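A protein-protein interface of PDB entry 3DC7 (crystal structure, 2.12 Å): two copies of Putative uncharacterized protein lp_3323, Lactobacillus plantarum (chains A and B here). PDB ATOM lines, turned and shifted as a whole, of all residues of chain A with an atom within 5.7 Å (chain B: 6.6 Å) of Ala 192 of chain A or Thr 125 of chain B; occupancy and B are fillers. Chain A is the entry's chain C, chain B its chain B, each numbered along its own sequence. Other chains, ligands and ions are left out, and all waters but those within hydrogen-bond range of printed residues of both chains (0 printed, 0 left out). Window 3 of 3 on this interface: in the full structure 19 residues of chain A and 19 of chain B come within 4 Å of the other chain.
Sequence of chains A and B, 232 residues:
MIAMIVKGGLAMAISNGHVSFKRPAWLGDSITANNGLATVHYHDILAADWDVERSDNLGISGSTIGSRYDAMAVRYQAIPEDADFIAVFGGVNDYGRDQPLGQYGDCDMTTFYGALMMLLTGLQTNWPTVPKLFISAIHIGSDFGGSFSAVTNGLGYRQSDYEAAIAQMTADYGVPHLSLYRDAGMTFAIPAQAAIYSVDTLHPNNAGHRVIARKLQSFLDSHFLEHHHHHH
Of the printed residues of chain B, Ile 190 of chain A touches Gln 124 and Thr 125. Of the printed residues of chain B, Ala 192 of chain A touches Thr 125 (3.2 Å) and Pro 128 (3.97 Å). Thr 121 of chain B touches none of the printed residues of chain A. Leu 123 of chain B touches none of the printed residues of chain A. Of the printed residues of chain A, Gln 124 of chain B touches Ile 190 and Gln 193. Of chain A, only Ile 190 and Ala 192 come within 4 Å of Thr 125 of chain B. Of the printed residues of chain A, Pro 128 of chain B touches Ala 192, Gln 193 and Ile 196. Printed residues of chain A within 4 Å of Thr 129 of chain B: Ile 196 (3.7 Å). The nearest residue of chain A that does not touch Thr 125 of chain B is Gln 193 of chain A (5.6 Å).
No position is printed for both chains. Of the 8 pairs that touch across the chains among the printed residues, none has its exchanged pair printed and touching as well.
Along chain B the printed residues that touch a printed residue of chain A span positions 124 to 129. Of the 7 printed residues of chain A, 4 touch a printed residue of chain B. Among the printed residues, 8 pairs touch across the chains.
The backbone carbonyl oxygen (O) of Pro 128 of chain B lies close to the side-chain amide oxygen (OE1) of Gln 193 of chain A, at 2.9 Å. The side-chain amide nitrogen (NE2) of Gln 124 of chain B lies within hydrogen-bond range of the side-chain amide oxygen (OE1) of Gln 193 of chain A (3.2 Å).
The side-chain hydroxyl (OG1) of Thr 125 of chain B lies within hydrogen-bond range of the backbone carbonyl oxygen (O) of Thr 121 of chain B (2.8 Å).
Among the printed residues, merely in contact across the chains: Ile 190 of chain A with Gln 124 of chain B, Ile 190 of chain A with Thr 125 of chain B, Ala 192 of chain A with Thr 125 of chain B, Ala 192 of chain A with Pro 128 of chain B, Ile 196 of chain A with Pro 128 of chain B and Ile 196 of chain A with Thr 129 of chain B.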
ATOM      1  N   ILE A 190      -0.161  -5.858  29.502  1.00  0.00           N
ATOM      2  CA  ILE A 190      -1.427  -5.202  29.851  1.00  0.00           C
ATOM      3  C   ILE A 190      -1.976  -5.878  31.095  1.00  0.00           C
ATOM      4  O   ILE A 190      -2.265  -7.075  31.064  1.00  0.00           O
ATOM      5  CB  ILE A 190      -2.485  -5.244  28.691  1.00  0.00           C
ATOM      6  CG1 ILE A 190      -1.955  -4.570  27.412  1.00  0.00           C
ATOM      7  CG2 ILE A 190      -3.828  -4.640  29.120  1.00  0.00           C
ATOM      8  CD1 ILE A 190      -1.935  -3.015  27.388  1.00  0.00           C
ATOM      9  N   PRO A 191      -2.093  -5.129  32.212  1.00  0.00           N
ATOM     10  CA  PRO A 191      -2.536  -5.731  33.470  1.00  0.00           C
ATOM     11  C   PRO A 191      -3.890  -6.436  33.414  1.00  0.00           C
ATOM     12  O   PRO A 191      -4.034  -7.504  33.998  1.00  0.00           O
ATOM     13  CB  PRO A 191      -2.565  -4.540  34.439  1.00  0.00           C
ATOM     14  CG  PRO A 191      -1.572  -3.599  33.876  1.00  0.00           C
ATOM     15  CD  PRO A 191      -1.777  -3.702  32.386  1.00  0.00           C
ATOM     16  N   ALA A 192      -4.870  -5.876  32.717  1.00  0.00           N
ATOM     17  CA  ALA A 192      -6.175  -6.542  32.608  1.00  0.00           C
ATOM     18  C   ALA A 192      -6.053  -7.983  32.077  1.00  0.00           C
ATOM     19  O   ALA A 192      -6.767  -8.873  32.534  1.00  0.00           O
ATOM     20  CB  ALA A 192      -7.135  -5.728  31.757  1.00  0.00           C
ATOM     21  N   GLN A 193      -5.125  -8.212  31.150  1.00  0.00           N
ATOM     22  CA  GLN A 193      -4.877  -9.552  30.599  1.00  0.00           C
ATOM     23  C   GLN A 193      -3.874 -10.402  31.386  1.00  0.00           C
ATOM     24  O   GLN A 193      -4.049 -11.628  31.500  1.00  0.00           O
ATOM     25  CB  GLN A 193      -4.442  -9.460  29.144  1.00  0.00           C
ATOM     26  CG  GLN A 193      -5.444  -8.747  28.290  1.00  0.00           C
ATOM     27  CD  GLN A 193      -5.131  -8.868  26.824  1.00  0.00           C
ATOM     28  OE1 GLN A 193      -5.950  -9.376  26.044  1.00  0.00           O
ATOM     29  NE2 GLN A 193      -3.933  -8.424  26.433  1.00  0.00           N
ATOM     30  N   ALA A 194      -2.824  -9.773  31.918  1.00  0.00           N
ATOM     31  CA  ALA A 194      -1.924 -10.477  32.831  1.00  0.00           C
ATOM     32  C   ALA A 194      -2.668 -11.012  34.066  1.00  0.00           C
ATOM     33  O   ALA A 194      -2.352 -12.095  34.559  1.00  0.00           O
ATOM     34  CB  ALA A 194      -0.757  -9.591  33.250  1.00  0.00           C
ATOM     35  N   ALA A 195      -3.654 -10.265  34.557  1.00  0.00           N
ATOM     36  CA  ALA A 195      -4.451 -10.715  35.696  1.00  0.00           C
ATOM     37  C   ALA A 195      -5.327 -11.923  35.371  1.00  0.00           C
ATOM     38  O   ALA A 195      -5.694 -12.671  36.260  1.00  0.00           O
ATOM     39  CB  ALA A 195      -5.316  -9.580  36.236  1.00  0.00           C
ATOM     40  N   ILE A 196      -5.668 -12.119  34.105  1.00  0.00           N
ATOM     41  CA  ILE A 196      -6.589 -13.202  33.750  1.00  0.00           C
ATOM     42  C   ILE A 196      -5.822 -14.447  33.326  1.00  0.00           C
ATOM     43  O   ILE A 196      -6.188 -15.575  33.697  1.00  0.00           O
ATOM     44  CB  ILE A 196      -7.574 -12.750  32.655  1.00  0.00           C
ATOM     45  CG1 ILE A 196      -8.490 -11.667  33.216  1.00  0.00           C
ATOM     46  CG2 ILE A 196      -8.401 -13.930  32.105  1.00  0.00           C
ATOM     47  CD1 ILE A 196      -9.280 -10.914  32.166  1.00  0.00           C
ATOM     48  N   LEU B 120      -4.812   0.353  20.870  1.00  0.00           N
ATOM     49  CA  LEU B 120      -4.488  -1.013  21.287  1.00  0.00           C
ATOM     50  C   LEU B 120      -4.474  -1.202  22.798  1.00  0.00           C
ATOM     51  O   LEU B 120      -5.004  -2.191  23.297  1.00  0.00           O
ATOM     52  CB  LEU B 120      -3.151  -1.447  20.687  1.00  0.00           C
ATOM     53  CG  LEU B 120      -3.327  -1.858  19.235  1.00  0.00           C
ATOM     54  CD1 LEU B 120      -2.019  -1.695  18.476  1.00  0.00           C
ATOM     55  CD2 LEU B 120      -3.901  -3.298  19.185  1.00  0.00           C
ATOM     56  N   THR B 121      -3.863  -0.255  23.514  1.00  0.00           N
ATOM     57  CA  THR B 121      -3.905  -0.261  24.978  1.00  0.00           C
ATOM     58  C   THR B 121      -5.354  -0.233  25.437  1.00  0.00           C
ATOM     59  O   THR B 121      -5.757  -1.057  26.255  1.00  0.00           O
ATOM     60  CB  THR B 121      -3.112   0.911  25.581  1.00  0.00           C
ATOM     61  OG1 THR B 121      -1.743   0.784  25.197  1.00  0.00           O
ATOM     62  CG2 THR B 121      -3.188   0.920  27.103  1.00  0.00           C
ATOM     63  N   GLY B 122      -6.139   0.689  24.888  1.00  0.00           N
ATOM     64  CA  GLY B 122      -7.565   0.763  25.200  1.00  0.00           C
ATOM     65  C   GLY B 122      -8.320  -0.538  24.987  1.00  0.00           C
ATOM     66  O   GLY B 122      -9.026  -0.998  25.875  1.00  0.00           O
ATOM     67  N   LEU B 123      -8.161  -1.147  23.818  1.00  0.00           N
ATOM     68  CA  LEU B 123      -8.906  -2.358  23.497  1.00  0.00           C
ATOM     69  C   LEU B 123      -8.537  -3.516  24.405  1.00  0.00           C
ATOM     70  O   LEU B 123      -9.411  -4.247  24.863  1.00  0.00           O
ATOM     71  CB  LEU B 123      -8.714  -2.763  22.028  1.00  0.00           C
ATOM     72  CG  LEU B 123      -9.273  -1.792  20.993  1.00  0.00           C
ATOM     73  CD1 LEU B 123      -8.747  -2.155  19.601  1.00  0.00           C
ATOM     74  CD2 LEU B 123     -10.825  -1.753  21.028  1.00  0.00           C
ATOM     75  N   GLN B 124      -7.245  -3.679  24.675  1.00  0.00           N
ATOM     76  CA  GLN B 124      -6.792  -4.831  25.452  1.00  0.00           C
ATOM     77  C   GLN B 124      -7.077  -4.649  26.950  1.00  0.00           C
ATOM     78  O   GLN B 124      -7.350  -5.619  27.653  1.00  0.00           O
ATOM     79  CB  GLN B 124      -5.315  -5.144  25.182  1.00  0.00           C
ATOM     80  CG  GLN B 124      -4.990  -5.580  23.729  1.00  0.00           C
ATOM     81  CD  GLN B 124      -5.374  -7.023  23.421  1.00  0.00           C
ATOM     82  OE1 GLN B 124      -4.537  -7.825  22.985  1.00  0.00           O
ATOM     83  NE2 GLN B 124      -6.621  -7.365  23.653  1.00  0.00           N
ATOM     84  N   THR B 125      -7.029  -3.402  27.417  1.00  0.00           N
ATOM     85  CA  THR B 125      -7.396  -3.045  28.793  1.00  0.00           C
ATOM     86  C   THR B 125      -8.875  -3.319  29.081  1.00  0.00           C
ATOM     87  O   THR B 125      -9.218  -3.902  30.100  1.00  0.00           O
ATOM     88  CB  THR B 125      -7.143  -1.542  29.033  1.00  0.00           C
ATOM     89  OG1 THR B 125      -5.737  -1.287  29.006  1.00  0.00           O
ATOM     90  CG2 THR B 125      -7.717  -1.064  30.372  1.00  0.00           C
ATOM     91  N   ASN B 126      -9.747  -2.890  28.182  1.00  0.00           N
ATOM     92  CA  ASN B 126     -11.182  -2.938  28.433  1.00  0.00           C
ATOM     93  C   ASN B 126     -11.885  -4.229  27.992  1.00  0.00           C
ATOM     94  O   ASN B 126     -12.873  -4.631  28.614  1.00  0.00           O
ATOM     95  CB  ASN B 126     -11.860  -1.699  27.840  1.00  0.00           C
ATOM     96  CG  ASN B 126     -11.241  -0.398  28.339  1.00  0.00           C
ATOM     97  OD1 ASN B 126     -11.353  -0.052  29.510  1.00  0.00           O
ATOM     98  ND2 ASN B 126     -10.595   0.333  27.442  1.00  0.00           N
ATOM     99  N   TRP B 127     -11.384  -4.869  26.928  1.00  0.00           N
ATOM    100  CA  TRP B 127     -11.958  -6.131  26.431  1.00  0.00           C
ATOM    101  C   TRP B 127     -10.918  -7.255  26.442  1.00  0.00           C
ATOM    102  O   TRP B 127     -10.619  -7.842  25.393  1.00  0.00           O
ATOM    103  CB  TRP B 127     -12.545  -5.971  25.022  1.00  0.00           C
ATOM    104  CG  TRP B 127     -13.680  -5.016  24.987  1.00  0.00           C
ATOM    105  CD1 TRP B 127     -15.022  -5.299  25.141  1.00  0.00           C
ATOM    106  CD2 TRP B 127     -13.583  -3.597  24.829  1.00  0.00           C
ATOM    107  NE1 TRP B 127     -15.752  -4.136  25.082  1.00  0.00           N
ATOM    108  CE2 TRP B 127     -14.895  -3.079  24.887  1.00  0.00           C
ATOM    109  CE3 TRP B 127     -12.510  -2.710  24.628  1.00  0.00           C
ATOM    110  CZ2 TRP B 127     -15.163  -1.708  24.758  1.00  0.00           C
ATOM    111  CZ3 TRP B 127     -12.783  -1.345  24.498  1.00  0.00           C
ATOM    112  CH2 TRP B 127     -14.094  -0.863  24.565  1.00  0.00           C
ATOM    113  N   PRO B 128     -10.375  -7.569  27.633  1.00  0.00           N
ATOM    114  CA  PRO B 128      -9.214  -8.445  27.695  1.00  0.00           C
ATOM    115  C   PRO B 128      -9.447  -9.861  27.185  1.00  0.00           C
ATOM    116  O   PRO B 128      -8.507 -10.484  26.703  1.00  0.00           O
ATOM    117  CB  PRO B 128      -8.861  -8.465  29.189  1.00  0.00           C
ATOM    118  CG  PRO B 128     -10.123  -8.101  29.882  1.00  0.00           C
ATOM    119  CD  PRO B 128     -10.806  -7.137  28.979  1.00  0.00           C
ATOM    120  N   THR B 129     -10.678 -10.359  27.292  1.00  0.00           N
ATOM    121  CA  THR B 129     -10.965 -11.753  26.936  1.00  0.00           C
ATOM    122  C   THR B 129     -11.621 -11.886  25.554  1.00  0.00           C
ATOM    123  O   THR B 129     -11.981 -12.980  25.136  1.00  0.00           O
ATOM    124  CB  THR B 129     -11.884 -12.398  27.964  1.00  0.00           C
ATOM    125  OG1 THR B 129     -13.197 -11.830  27.829  1.00  0.00           O
ATOM    126  CG2 THR B 129     -11.353 -12.139  29.386  1.00  0.00           C
